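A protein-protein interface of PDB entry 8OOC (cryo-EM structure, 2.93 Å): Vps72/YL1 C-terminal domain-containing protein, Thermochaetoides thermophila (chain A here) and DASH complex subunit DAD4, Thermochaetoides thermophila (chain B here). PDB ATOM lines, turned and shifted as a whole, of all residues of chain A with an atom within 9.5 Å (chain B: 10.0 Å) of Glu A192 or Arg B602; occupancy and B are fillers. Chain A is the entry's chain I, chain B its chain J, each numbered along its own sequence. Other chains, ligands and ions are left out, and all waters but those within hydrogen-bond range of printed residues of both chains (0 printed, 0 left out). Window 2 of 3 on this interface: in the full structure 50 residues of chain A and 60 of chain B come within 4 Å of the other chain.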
ATOM      1  N   CYS A 170       4.059  -7.698  29.639  1.00  0.00           N
ATOM      2  CA  CYS A 170       2.666  -7.785  30.060  1.00  0.00           C
ATOM      3  C   CYS A 170       2.145  -9.211  29.945  1.00  0.00           C
ATOM      4  O   CYS A 170       2.261  -9.845  28.893  1.00  0.00           O
ATOM      5  CB  CYS A 170       1.807  -6.841  29.218  1.00  0.00           C
ATOM      6  SG  CYS A 170       0.029  -6.950  29.522  1.00  0.00           S
ATOM      7  N   VAL A 172      -0.887 -10.206  29.888  1.00  0.00           N
ATOM      8  CA  VAL A 172      -2.004 -10.254  28.953  1.00  0.00           C
ATOM      9  C   VAL A 172      -1.494 -10.200  27.518  1.00  0.00           C
ATOM     10  O   VAL A 172      -1.547 -11.202  26.798  1.00  0.00           O
ATOM     11  CB  VAL A 172      -3.004  -9.115  29.225  1.00  0.00           C
ATOM     12  CG1 VAL A 172      -4.173  -9.192  28.260  1.00  0.00           C
ATOM     13  CG2 VAL A 172      -3.486  -9.179  30.661  1.00  0.00           C
ATOM     14  N   THR A 173      -1.005  -9.039  27.088  1.00  0.00           N
ATOM     15  CA  THR A 173      -0.727  -8.794  25.679  1.00  0.00           C
ATOM     16  C   THR A 173       0.731  -9.016  25.291  1.00  0.00           C
ATOM     17  O   THR A 173       1.076  -8.829  24.122  1.00  0.00           O
ATOM     18  CB  THR A 173      -1.136  -7.367  25.308  1.00  0.00           C
ATOM     19  OG1 THR A 173      -1.040  -7.188  23.889  1.00  0.00           O
ATOM     20  CG2 THR A 173      -0.226  -6.372  25.995  1.00  0.00           C
ATOM     21  N   LEU A 175       3.225  -7.292  25.374  1.00  0.00           N
ATOM     22  CA  LEU A 175       3.958  -6.040  25.241  1.00  0.00           C
ATOM     23  C   LEU A 175       4.750  -5.735  26.512  1.00  0.00           C
ATOM     24  O   LEU A 175       4.469  -6.292  27.576  1.00  0.00           O
ATOM     25  CB  LEU A 175       2.987  -4.903  24.927  1.00  0.00           C
ATOM     26  CG  LEU A 175       2.194  -5.028  23.628  1.00  0.00           C
ATOM     27  CD1 LEU A 175       1.364  -3.784  23.394  1.00  0.00           C
ATOM     28  CD2 LEU A 175       3.121  -5.286  22.453  1.00  0.00           C
ATOM     29  N   TYR A 179       4.564  -1.803  34.674  1.00  0.00           N
ATOM     30  CA  TYR A 179       3.781  -1.869  35.897  1.00  0.00           C
ATOM     31  C   TYR A 179       3.555  -3.312  36.324  1.00  0.00           C
ATOM     32  O   TYR A 179       3.323  -4.192  35.491  1.00  0.00           O
ATOM     33  CB  TYR A 179       2.429  -1.192  35.688  1.00  0.00           C
ATOM     34  CG  TYR A 179       2.503   0.121  34.944  1.00  0.00           C
ATOM     35  CD1 TYR A 179       3.148   1.221  35.491  1.00  0.00           C
ATOM     36  CD2 TYR A 179       1.943   0.251  33.683  1.00  0.00           C
ATOM     37  CE1 TYR A 179       3.275   2.394  34.783  1.00  0.00           C
ATOM     38  CE2 TYR A 179       2.021   1.436  32.988  1.00  0.00           C
ATOM     39  CZ  TYR A 179       2.698   2.502  33.537  1.00  0.00           C
ATOM     40  OH  TYR A 179       2.720   3.699  32.867  1.00  0.00           O
ATOM     41  N   TYR A 188       1.346  -5.651  33.462  1.00  0.00           N
ATOM     42  CA  TYR A 188       0.450  -5.074  32.476  1.00  0.00           C
ATOM     43  C   TYR A 188       1.070  -3.865  31.795  1.00  0.00           C
ATOM     44  O   TYR A 188       1.924  -3.174  32.353  1.00  0.00           O
ATOM     45  CB  TYR A 188      -0.901  -4.728  33.118  1.00  0.00           C
ATOM     46  CG  TYR A 188      -0.853  -3.657  34.182  1.00  0.00           C
ATOM     47  CD1 TYR A 188      -0.576  -3.988  35.501  1.00  0.00           C
ATOM     48  CD2 TYR A 188      -1.102  -2.328  33.879  1.00  0.00           C
ATOM     49  CE1 TYR A 188      -0.535  -3.027  36.485  1.00  0.00           C
ATOM     50  CE2 TYR A 188      -1.064  -1.355  34.861  1.00  0.00           C
ATOM     51  CZ  TYR A 188      -0.782  -1.713  36.162  1.00  0.00           C
ATOM     52  OH  TYR A 188      -0.742  -0.760  37.152  1.00  0.00           O
ATOM     53  N   HIS A 189       0.609  -3.627  30.566  1.00  0.00           N
ATOM     54  CA  HIS A 189       1.164  -2.602  29.691  1.00  0.00           C
ATOM     55  C   HIS A 189       0.647  -1.211  30.036  1.00  0.00           C
ATOM     56  O   HIS A 189       1.426  -0.257  30.120  1.00  0.00           O
ATOM     57  CB  HIS A 189       0.849  -2.946  28.235  1.00  0.00           C
ATOM     58  CG  HIS A 189       1.441  -1.996  27.245  1.00  0.00           C
ATOM     59  ND1 HIS A 189       2.799  -1.822  27.099  1.00  0.00           N
ATOM     60  CD2 HIS A 189       0.859  -1.174  26.340  1.00  0.00           C
ATOM     61  CE1 HIS A 189       3.029  -0.931  26.152  1.00  0.00           C
ATOM     62  NE2 HIS A 189       1.867  -0.522  25.674  1.00  0.00           N
ATOM     63  N   ASN A 190      -0.661  -1.072  30.237  1.00  0.00           N
ATOM     64  CA  ASN A 190      -1.271   0.247  30.358  1.00  0.00           C
ATOM     65  C   ASN A 190      -2.588   0.135  31.120  1.00  0.00           C
ATOM     66  O   ASN A 190      -3.009  -0.949  31.526  1.00  0.00           O
ATOM     67  CB  ASN A 190      -1.441   0.898  28.976  1.00  0.00           C
ATOM     68  CG  ASN A 190      -2.472   0.194  28.098  1.00  0.00           C
ATOM     69  OD1 ASN A 190      -3.198  -0.693  28.537  1.00  0.00           O
ATOM     70  ND2 ASN A 190      -2.532   0.603  26.837  1.00  0.00           N
ATOM     71  N   LYS A 191      -3.225   1.292  31.317  1.00  0.00           N
ATOM     72  CA  LYS A 191      -4.495   1.373  32.035  1.00  0.00           C
ATOM     73  C   LYS A 191      -5.610   0.574  31.367  1.00  0.00           C
ATOM     74  O   LYS A 191      -6.495   0.059  32.059  1.00  0.00           O
ATOM     75  CB  LYS A 191      -4.902   2.840  32.191  1.00  0.00           C
ATOM     76  CG  LYS A 191      -5.256   3.542  30.891  1.00  0.00           C
ATOM     77  CD  LYS A 191      -5.730   4.962  31.151  1.00  0.00           C
ATOM     78  CE  LYS A 191      -6.121   5.662  29.861  1.00  0.00           C
ATOM     79  NZ  LYS A 191      -6.630   7.042  30.104  1.00  0.00           N
ATOM     80  N   GLU A 192      -5.597   0.464  30.038  1.00  0.00           N
ATOM     81  CA  GLU A 192      -6.613  -0.337  29.356  1.00  0.00           C
ATOM     82  C   GLU A 192      -6.543  -1.803  29.767  1.00  0.00           C
ATOM     83  O   GLU A 192      -7.578  -2.458  29.929  1.00  0.00           O
ATOM     84  CB  GLU A 192      -6.460  -0.194  27.841  1.00  0.00           C
ATOM     85  CG  GLU A 192      -7.356  -1.120  27.041  1.00  0.00           C
ATOM     86  CD  GLU A 192      -7.580  -0.636  25.626  1.00  0.00           C
ATOM     87  OE1 GLU A 192      -6.621  -0.117  25.018  1.00  0.00           O
ATOM     88  OE2 GLU A 192      -8.715  -0.776  25.123  1.00  0.00           O
ATOM     89  N   ILE A 193      -5.336  -2.335  29.946  1.00  0.00           N
ATOM     90  CA  ILE A 193      -5.180  -3.730  30.347  1.00  0.00           C
ATOM     91  C   ILE A 193      -5.388  -3.901  31.850  1.00  0.00           C
ATOM     92  O   ILE A 193      -5.939  -4.909  32.301  1.00  0.00           O
ATOM     93  CB  ILE A 193      -3.804  -4.244  29.888  1.00  0.00           C
ATOM     94  CG1 ILE A 193      -3.792  -4.393  28.367  1.00  0.00           C
ATOM     95  CG2 ILE A 193      -3.461  -5.563  30.554  1.00  0.00           C
ATOM     96  CD1 ILE A 193      -2.448  -4.186  27.746  1.00  0.00           C
ATOM     97  N   PHE A 194      -4.953  -2.925  32.646  1.00  0.00           N
ATOM     98  CA  PHE A 194      -5.302  -2.902  34.066  1.00  0.00           C
ATOM     99  C   PHE A 194      -6.813  -2.938  34.286  1.00  0.00           C
ATOM    100  O   PHE A 194      -7.297  -3.600  35.213  1.00  0.00           O
ATOM    101  CB  PHE A 194      -4.695  -1.660  34.717  1.00  0.00           C
ATOM    102  CG  PHE A 194      -4.931  -1.565  36.196  1.00  0.00           C
ATOM    103  CD1 PHE A 194      -4.052  -2.150  37.086  1.00  0.00           C
ATOM    104  CD2 PHE A 194      -6.020  -0.875  36.698  1.00  0.00           C
ATOM    105  CE1 PHE A 194      -4.260  -2.059  38.450  1.00  0.00           C
ATOM    106  CE2 PHE A 194      -6.233  -0.781  38.060  1.00  0.00           C
ATOM    107  CZ  PHE A 194      -5.351  -1.374  38.936  1.00  0.00           C
ATOM    108  N   ALA A 195      -7.572  -2.224  33.451  1.00  0.00           N
ATOM    109  CA  ALA A 195      -9.030  -2.251  33.537  1.00  0.00           C
ATOM    110  C   ALA A 195      -9.620  -3.644  33.329  1.00  0.00           C
ATOM    111  O   ALA A 195     -10.549  -4.039  34.043  1.00  0.00           O
ATOM    112  CB  ALA A 195      -9.621  -1.275  32.522  1.00  0.00           C
ATOM    113  N   MET A 196      -9.104  -4.408  32.362  1.00  0.00           N
ATOM    114  CA  MET A 196      -9.565  -5.788  32.202  1.00  0.00           C
ATOM    115  C   MET A 196      -9.040  -6.712  33.298  1.00  0.00           C
ATOM    116  O   MET A 196      -9.746  -7.634  33.723  1.00  0.00           O
ATOM    117  CB  MET A 196      -9.196  -6.309  30.809  1.00  0.00           C
ATOM    118  CG  MET A 196      -7.740  -6.685  30.606  1.00  0.00           C
ATOM    119  SD  MET A 196      -7.493  -8.062  29.467  1.00  0.00           S
ATOM    120  CE  MET A 196      -7.550  -9.452  30.587  1.00  0.00           C
ATOM    121  N   ILE A 197      -7.808  -6.499  33.761  1.00  0.00           N
ATOM    122  CA  ILE A 197      -7.237  -7.361  34.797  1.00  0.00           C
ATOM    123  C   ILE A 197      -8.061  -7.307  36.078  1.00  0.00           C
ATOM    124  O   ILE A 197      -8.395  -8.343  36.665  1.00  0.00           O
ATOM    125  CB  ILE A 197      -5.766  -6.995  35.055  1.00  0.00           C
ATOM    126  CG1 ILE A 197      -4.891  -7.510  33.916  1.00  0.00           C
ATOM    127  CG2 ILE A 197      -5.298  -7.559  36.381  1.00  0.00           C
ATOM    128  CD1 ILE A 197      -3.501  -6.961  33.944  1.00  0.00           C
ATOM    129  N   ARG A 198      -8.407  -6.103  36.531  1.00  0.00           N
ATOM    130  CA  ARG A 198      -9.137  -5.954  37.785  1.00  0.00           C
ATOM    131  C   ARG A 198     -10.592  -6.406  37.709  1.00  0.00           C
ATOM    132  O   ARG A 198     -11.254  -6.454  38.749  1.00  0.00           O
ATOM    133  CB  ARG A 198      -9.066  -4.503  38.259  1.00  0.00           C
ATOM    134  CG  ARG A 198      -7.711  -4.122  38.830  1.00  0.00           C
ATOM    135  CD  ARG A 198      -7.426  -4.863  40.128  1.00  0.00           C
ATOM    136  NE  ARG A 198      -6.185  -4.423  40.754  1.00  0.00           N
ATOM    137  CZ  ARG A 198      -6.110  -3.560  41.758  1.00  0.00           C
ATOM    138  NH1 ARG A 198      -7.192  -2.988  42.261  1.00  0.00           N
ATOM    139  NH2 ARG A 198      -4.918  -3.250  42.260  1.00  0.00           N
ATOM    140  N   ASN A 199     -11.109  -6.735  36.525  1.00  0.00           N
ATOM    141  CA  ASN A 199     -12.449  -7.297  36.401  1.00  0.00           C
ATOM    142  C   ASN A 199     -12.455  -8.638  35.666  1.00  0.00           C
ATOM    143  O   ASN A 199     -13.466  -9.036  35.085  1.00  0.00           O
ATOM    144  CB  ASN A 199     -13.395  -6.272  35.762  1.00  0.00           C
ATOM    145  CG  ASN A 199     -13.235  -6.131  34.242  1.00  0.00           C
ATOM    146  OD1 ASN A 199     -12.690  -6.989  33.549  1.00  0.00           O
ATOM    147  ND2 ASN A 199     -13.734  -5.016  33.724  1.00  0.00           N
ATOM    148  N   TYR B 251     -10.091 -16.124  26.164  1.00  0.00           N
ATOM    149  CA  TYR B 251     -10.564 -16.672  27.429  1.00  0.00           C
ATOM    150  C   TYR B 251     -12.073 -16.545  27.587  1.00  0.00           C
ATOM    151  O   TYR B 251     -12.670 -17.295  28.367  1.00  0.00           O
ATOM    152  CB  TYR B 251      -9.860 -15.970  28.587  1.00  0.00           C
ATOM    153  CG  TYR B 251     -10.375 -14.575  28.866  1.00  0.00           C
ATOM    154  CD1 TYR B 251      -9.888 -13.480  28.164  1.00  0.00           C
ATOM    155  CD2 TYR B 251     -11.337 -14.350  29.842  1.00  0.00           C
ATOM    156  CE1 TYR B 251     -10.353 -12.206  28.417  1.00  0.00           C
ATOM    157  CE2 TYR B 251     -11.810 -13.080  30.101  1.00  0.00           C
ATOM    158  CZ  TYR B 251     -11.313 -12.012  29.386  1.00  0.00           C
ATOM    159  OH  TYR B 251     -11.782 -10.745  29.641  1.00  0.00           O
ATOM    160  N   LEU B 285       1.503  -3.657  17.811  1.00  0.00           N
ATOM    161  CA  LEU B 285       0.057  -3.471  17.773  1.00  0.00           C
ATOM    162  C   LEU B 285      -0.367  -2.053  17.401  1.00  0.00           C
ATOM    163  O   LEU B 285      -1.515  -1.674  17.654  1.00  0.00           O
ATOM    164  CB  LEU B 285      -0.557  -3.869  19.116  1.00  0.00           C
ATOM    165  CG  LEU B 285      -0.424  -5.343  19.505  1.00  0.00           C
ATOM    166  CD1 LEU B 285      -1.131  -5.626  20.816  1.00  0.00           C
ATOM    167  CD2 LEU B 285      -0.966  -6.232  18.403  1.00  0.00           C
ATOM    168  N   TRP B 287      -1.975   0.283  14.919  1.00  0.00           N
ATOM    169  CA  TRP B 287      -2.961   0.023  13.870  1.00  0.00           C
ATOM    170  C   TRP B 287      -2.392   0.201  12.468  1.00  0.00           C
ATOM    171  O   TRP B 287      -2.810  -0.500  11.540  1.00  0.00           O
ATOM    172  CB  TRP B 287      -4.178   0.934  14.047  1.00  0.00           C
ATOM    173  CG  TRP B 287      -4.881   0.779  15.356  1.00  0.00           C
ATOM    174  CD1 TRP B 287      -4.639   1.471  16.506  1.00  0.00           C
ATOM    175  CD2 TRP B 287      -5.970  -0.107  15.644  1.00  0.00           C
ATOM    176  NE1 TRP B 287      -5.497   1.058  17.496  1.00  0.00           N
ATOM    177  CE2 TRP B 287      -6.326   0.092  16.990  1.00  0.00           C
ATOM    178  CE3 TRP B 287      -6.673  -1.053  14.893  1.00  0.00           C
ATOM    179  CZ2 TRP B 287      -7.353  -0.620  17.603  1.00  0.00           C
ATOM    180  CZ3 TRP B 287      -7.693  -1.759  15.502  1.00  0.00           C
ATOM    181  CH2 TRP B 287      -8.022  -1.539  16.845  1.00  0.00           C
ATOM    182  N   GLN B 601     -16.004   8.723  21.463  1.00  0.00           N
ATOM    183  CA  GLN B 601     -14.577   8.953  21.661  1.00  0.00           C
ATOM    184  C   GLN B 601     -13.910   7.746  22.311  1.00  0.00           C
ATOM    185  O   GLN B 601     -12.684   7.637  22.333  1.00  0.00           O
ATOM    186  CB  GLN B 601     -14.348  10.210  22.506  1.00  0.00           C
ATOM    187  CG  GLN B 601     -14.857  10.107  23.933  1.00  0.00           C
ATOM    188  CD  GLN B 601     -14.754  11.424  24.679  1.00  0.00           C
ATOM    189  OE1 GLN B 601     -14.084  12.354  24.229  1.00  0.00           O
ATOM    190  NE2 GLN B 601     -15.422  11.510  25.824  1.00  0.00           N
ATOM    191  N   ARG B 602     -14.725   6.841  22.844  1.00  0.00           N
ATOM    192  CA  ARG B 602     -14.278   5.514  23.247  1.00  0.00           C
ATOM    193  C   ARG B 602     -14.845   4.504  22.261  1.00  0.00           C
ATOM    194  O   ARG B 602     -16.065   4.326  22.185  1.00  0.00           O
ATOM    195  CB  ARG B 602     -14.739   5.206  24.672  1.00  0.00           C
ATOM    196  CG  ARG B 602     -14.508   3.780  25.139  1.00  0.00           C
ATOM    197  CD  ARG B 602     -13.040   3.402  25.119  1.00  0.00           C
ATOM    198  NE  ARG B 602     -12.835   2.044  25.610  1.00  0.00           N
ATOM    199  CZ  ARG B 602     -11.696   1.374  25.508  1.00  0.00           C
ATOM    200  NH1 ARG B 602     -10.627   1.910  24.944  1.00  0.00           N
ATOM    201  NH2 ARG B 602     -11.626   0.138  25.993  1.00  0.00           N
ATOM    202  N   ASP B 603     -13.963   3.847  21.512  1.00  0.00           N
ATOM    203  CA  ASP B 603     -14.377   2.965  20.431  1.00  0.00           C
ATOM    204  C   ASP B 603     -13.468   1.748  20.370  1.00  0.00           C
ATOM    205  O   ASP B 603     -12.349   1.750  20.889  1.00  0.00           O
ATOM    206  CB  ASP B 603     -14.371   3.688  19.080  1.00  0.00           C
ATOM    207  CG  ASP B 603     -15.491   4.696  18.957  1.00  0.00           C
ATOM    208  OD1 ASP B 603     -16.641   4.349  19.299  1.00  0.00           O
ATOM    209  OD2 ASP B 603     -15.224   5.832  18.516  1.00  0.00           O
ATOM    210  N   TRP B 604     -13.983   0.694  19.733  1.00  0.00           N
ATOM    211  CA  TRP B 604     -13.163  -0.470  19.410  1.00  0.00           C
ATOM    212  C   TRP B 604     -11.923  -0.076  18.614  1.00  0.00           C
ATOM    213  O   TRP B 604     -10.838  -0.633  18.822  1.00  0.00           O
ATOM    214  CB  TRP B 604     -14.006  -1.501  18.655  1.00  0.00           C
ATOM    215  CG  TRP B 604     -14.433  -1.077  17.278  1.00  0.00           C
ATOM    216  CD1 TRP B 604     -15.635  -0.538  16.928  1.00  0.00           C
ATOM    217  CD2 TRP B 604     -13.678  -1.191  16.064  1.00  0.00           C
ATOM    218  NE1 TRP B 604     -15.670  -0.290  15.579  1.00  0.00           N
ATOM    219  CE2 TRP B 604     -14.480  -0.683  15.025  1.00  0.00           C
ATOM    220  CE3 TRP B 604     -12.398  -1.662  15.757  1.00  0.00           C
ATOM    221  CZ2 TRP B 604     -14.047  -0.635  13.703  1.00  0.00           C
ATOM    222  CZ3 TRP B 604     -11.970  -1.613  14.445  1.00  0.00           C
ATOM    223  CH2 TRP B 604     -12.792  -1.105  13.433  1.00  0.00           C
ATOM    224  N   SER B 605     -12.064   0.882  17.697  1.00  0.00           N
ATOM    225  CA  SER B 605     -10.970   1.345  16.850  1.00  0.00           C
ATOM    226  C   SER B 605      -9.919   2.140  17.610  1.00  0.00           C
ATOM    227  O   SER B 605      -8.952   2.601  16.994  1.00  0.00           O
ATOM    228  CB  SER B 605     -11.521   2.190  15.702  1.00  0.00           C
ATOM    229  OG  SER B 605     -12.224   3.316  16.196  1.00  0.00           O
ATOM    230  N   LYS B 606     -10.080   2.310  18.919  1.00  0.00           N
ATOM    231  CA  LYS B 606      -9.068   2.927  19.766  1.00  0.00           C
ATOM    232  C   LYS B 606      -8.666   2.002  20.909  1.00  0.00           C
ATOM    233  O   LYS B 606      -7.982   2.435  21.845  1.00  0.00           O
ATOM    234  CB  LYS B 606      -9.586   4.271  20.297  1.00  0.00           C
ATOM    235  CG  LYS B 606      -8.523   5.219  20.837  1.00  0.00           C
ATOM    236  CD  LYS B 606      -7.499   5.557  19.765  1.00  0.00           C
ATOM    237  CE  LYS B 606      -6.587   6.692  20.207  1.00  0.00           C
ATOM    238  NZ  LYS B 606      -5.657   6.279  21.296  1.00  0.00           N
ATOM    239  N   SER B 607      -9.065   0.733  20.852  1.00  0.00           N
ATOM    240  CA  SER B 607      -8.796  -0.231  21.911  1.00  0.00           C
ATOM    241  C   SER B 607      -7.629  -1.124  21.508  1.00  0.00           C
ATOM    242  O   SER B 607      -7.665  -1.774  20.458  1.00  0.00           O
ATOM    243  CB  SER B 607     -10.037  -1.072  22.205  1.00  0.00           C
ATOM    244  OG  SER B 607      -9.759  -2.063  23.177  1.00  0.00           O
ATOM    245  N   LEU B 608      -6.598  -1.145  22.355  1.00  0.00           N
ATOM    246  CA  LEU B 608      -5.451  -2.024  22.150  1.00  0.00           C
ATOM    247  C   LEU B 608      -5.852  -3.495  22.193  1.00  0.00           C
ATOM    248  O   LEU B 608      -5.315  -4.316  21.440  1.00  0.00           O
ATOM    249  CB  LEU B 608      -4.386  -1.729  23.208  1.00  0.00           C
ATOM    250  CG  LEU B 608      -3.081  -2.525  23.144  1.00  0.00           C
ATOM    251  CD1 LEU B 608      -2.398  -2.305  21.810  1.00  0.00           C
ATOM    252  CD2 LEU B 608      -2.159  -2.143  24.290  1.00  0.00           C
ATOM    253  N   LEU B 609      -6.800  -3.842  23.062  1.00  0.00           N
ATOM    254  CA  LEU B 609      -7.254  -5.225  23.172  1.00  0.00           C
ATOM    255  C   LEU B 609      -8.102  -5.670  21.987  1.00  0.00           C
ATOM    256  O   LEU B 609      -8.160  -6.869  21.694  1.00  0.00           O
ATOM    257  CB  LEU B 609      -8.032  -5.414  24.471  1.00  0.00           C
ATOM    258  CG  LEU B 609      -7.186  -5.400  25.741  1.00  0.00           C
ATOM    259  CD1 LEU B 609      -8.073  -5.342  26.969  1.00  0.00           C
ATOM    260  CD2 LEU B 609      -6.281  -6.615  25.783  1.00  0.00           C
ATOM    261  N   HIS B 610      -8.764  -4.746  21.290  1.00  0.00           N
ATOM    262  CA  HIS B 610      -9.374  -5.118  20.016  1.00  0.00           C
ATOM    263  C   HIS B 610      -8.312  -5.442  18.972  1.00  0.00           C
ATOM    264  O   HIS B 610      -8.428  -6.436  18.245  1.00  0.00           O
ATOM    265  CB  HIS B 610     -10.289  -3.999  19.518  1.00  0.00           C
ATOM    266  CG  HIS B 610     -11.053  -4.358  18.282  1.00  0.00           C
ATOM    267  ND1 HIS B 610     -12.303  -4.933  18.320  1.00  0.00           N
ATOM    268  CD2 HIS B 610     -10.732  -4.243  16.971  1.00  0.00           C
ATOM    269  CE1 HIS B 610     -12.726  -5.145  17.087  1.00  0.00           C
ATOM    270  NE2 HIS B 610     -11.791  -4.736  16.249  1.00  0.00           N
ATOM    271  N   ALA B 611      -7.279  -4.606  18.871  1.00  0.00           N
ATOM    272  CA  ALA B 611      -6.164  -4.895  17.974  1.00  0.00           C
ATOM    273  C   ALA B 611      -5.512  -6.229  18.320  1.00  0.00           C
ATOM    274  O   ALA B 611      -5.213  -7.040  17.435  1.00  0.00           O
ATOM    275  CB  ALA B 611      -5.140  -3.763  18.034  1.00  0.00           C
ATOM    276  N   PHE B 612      -5.277  -6.458  19.613  1.00  0.00           N
ATOM    277  CA  PHE B 612      -4.702  -7.713  20.086  1.00  0.00           C
ATOM    278  C   PHE B 612      -5.514  -8.920  19.630  1.00  0.00           C
ATOM    279  O   PHE B 612      -4.947  -9.952  19.254  1.00  0.00           O
ATOM    280  CB  PHE B 612      -4.614  -7.670  21.613  1.00  0.00           C
ATOM    281  CG  PHE B 612      -4.092  -8.930  22.241  1.00  0.00           C
ATOM    282  CD1 PHE B 612      -2.850  -9.430  21.899  1.00  0.00           C
ATOM    283  CD2 PHE B 612      -4.838  -9.604  23.194  1.00  0.00           C
ATOM    284  CE1 PHE B 612      -2.363 -10.580  22.487  1.00  0.00           C
ATOM    285  CE2 PHE B 612      -4.358 -10.759  23.784  1.00  0.00           C
ATOM    286  CZ  PHE B 612      -3.118 -11.245  23.432  1.00  0.00           C
ATOM    287  N   ARG B 613      -6.841  -8.814  19.658  1.00  0.00           N
ATOM    288  CA  ARG B 613      -7.708  -9.964  19.444  1.00  0.00           C
ATOM    289  C   ARG B 613      -8.308 -10.032  18.047  1.00  0.00           C
ATOM    290  O   ARG B 613      -8.518 -11.135  17.533  1.00  0.00           O
ATOM    291  CB  ARG B 613      -8.828  -9.975  20.486  1.00  0.00           C
ATOM    292  CG  ARG B 613      -8.319 -10.262  21.885  1.00  0.00           C
ATOM    293  CD  ARG B 613      -9.409 -10.130  22.923  1.00  0.00           C
ATOM    294  NE  ARG B 613      -8.925 -10.475  24.253  1.00  0.00           N
ATOM    295  CZ  ARG B 613      -9.154  -9.756  25.342  1.00  0.00           C
ATOM    296  NH1 ARG B 613     -10.011  -8.749  25.338  1.00  0.00           N
ATOM    297  NH2 ARG B 613      -8.551 -10.091  26.478  1.00  0.00           N
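Of chain B, only Arg B602 (3.2 Å), Ser B607 (2.6 Å) and Leu B608 (2.9 Å) come within 4 Å of Glu A192.
Arg B602 touches just one residue of chain A: Glu A192.
Asn A190 touches just one residue of chain B: Leu B608 (3.8 Å).
No residue of chain B comes within 4 Å of Ile A193.
No residue of chain B comes within 4 Å of Ala A195.
Printed residues of chain B within 4 Å of Leu A175: Leu B608 (3.99 Å).
Printed residues of chain A within 4 Å of Leu B608: Leu A175, His A189, Asn A190 and Glu A192.
Of the printed residues of chain A, Leu B285 touches Thr A173.
Printed residues of chain A within 4 Å of Phe B612: Val A172 and Thr A173.
Of the printed residues of chain B, Met A196 touches Leu B609 (3.7 Å) and Arg B613 (3.8 Å).
Cys A170 touches none of the printed residues of chain B.
The nearest printed residue of chain A that does not touch Leu B285 is Leu A175 (4.03 Å).
Printed residues of chain A that touch a printed residue of chain B: Val A172, Thr A173, Leu A175, His A189, Asn A190, Glu A192 and Met A196.
Hydrophobic or aromatic side chains of chain A that line the printed part of chain B: Leu A175, His A189 and Met A196.
Along chain B the printed residues that touch a printed residue of chain A span positions 285 to 613.
Among the printed residues, 11 pairs touch across the chains.
Among the printed residues, Asp or Glu carboxylates within 4 Å of a Lys or Arg side-chain nitrogen of the other chain: Glu A192 with Arg B602 (3.2 Å).
NH2 of Arg B602 lies within salt-bridge range of OE2 of Glu A192 (3.2 Å).
NH2 of Arg B613 sits at hydrogen-bond distance from SD of Met A196 (3.8 Å).
OE2 of Glu A192 lies within hydrogen-bond range of OG of Ser B607 (2.6 Å).
The side-chain carboxylate (OE1) of Glu A192 is in hydrogen-bond range of the backbone NH (N) of Leu B608.
The side-chain sulfur (SG) of Cys A170 sits at hydrogen-bond distance from the backbone NH (N) of Thr A173 (3.4 Å).
N of Ile A193 lies within hydrogen-bond range of OD1 of Asn A190 (3.0 Å).
The side-chain hydroxyl (OG) of Ser B607 sits at hydrogen-bond distance from the backbone NH (N) of His B610 (3.4 Å).
The side-chain hydroxyl (OG) of Ser B607 lies close to the backbone NH (N) of Leu B609 (3.5 Å).
The backbone carbonyl oxygen of Leu A175 sits at hydrogen-bond distance from the backbone NH of Cys A170 (2.5 Å).
The side-chain sulfur (SG) of Cys A170 sits close to the backbone NH (N) of Val A172 (3.4 Å).
Among the printed residues, pairs that only touch across the chains: Val A172 with Phe B612, Thr A173 with Leu B285, Thr A173 with Phe B612, Leu A175 with Leu B608, His A189 with Leu B608, Asn A190 with Leu B608 and Met A196 with Leu B609.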
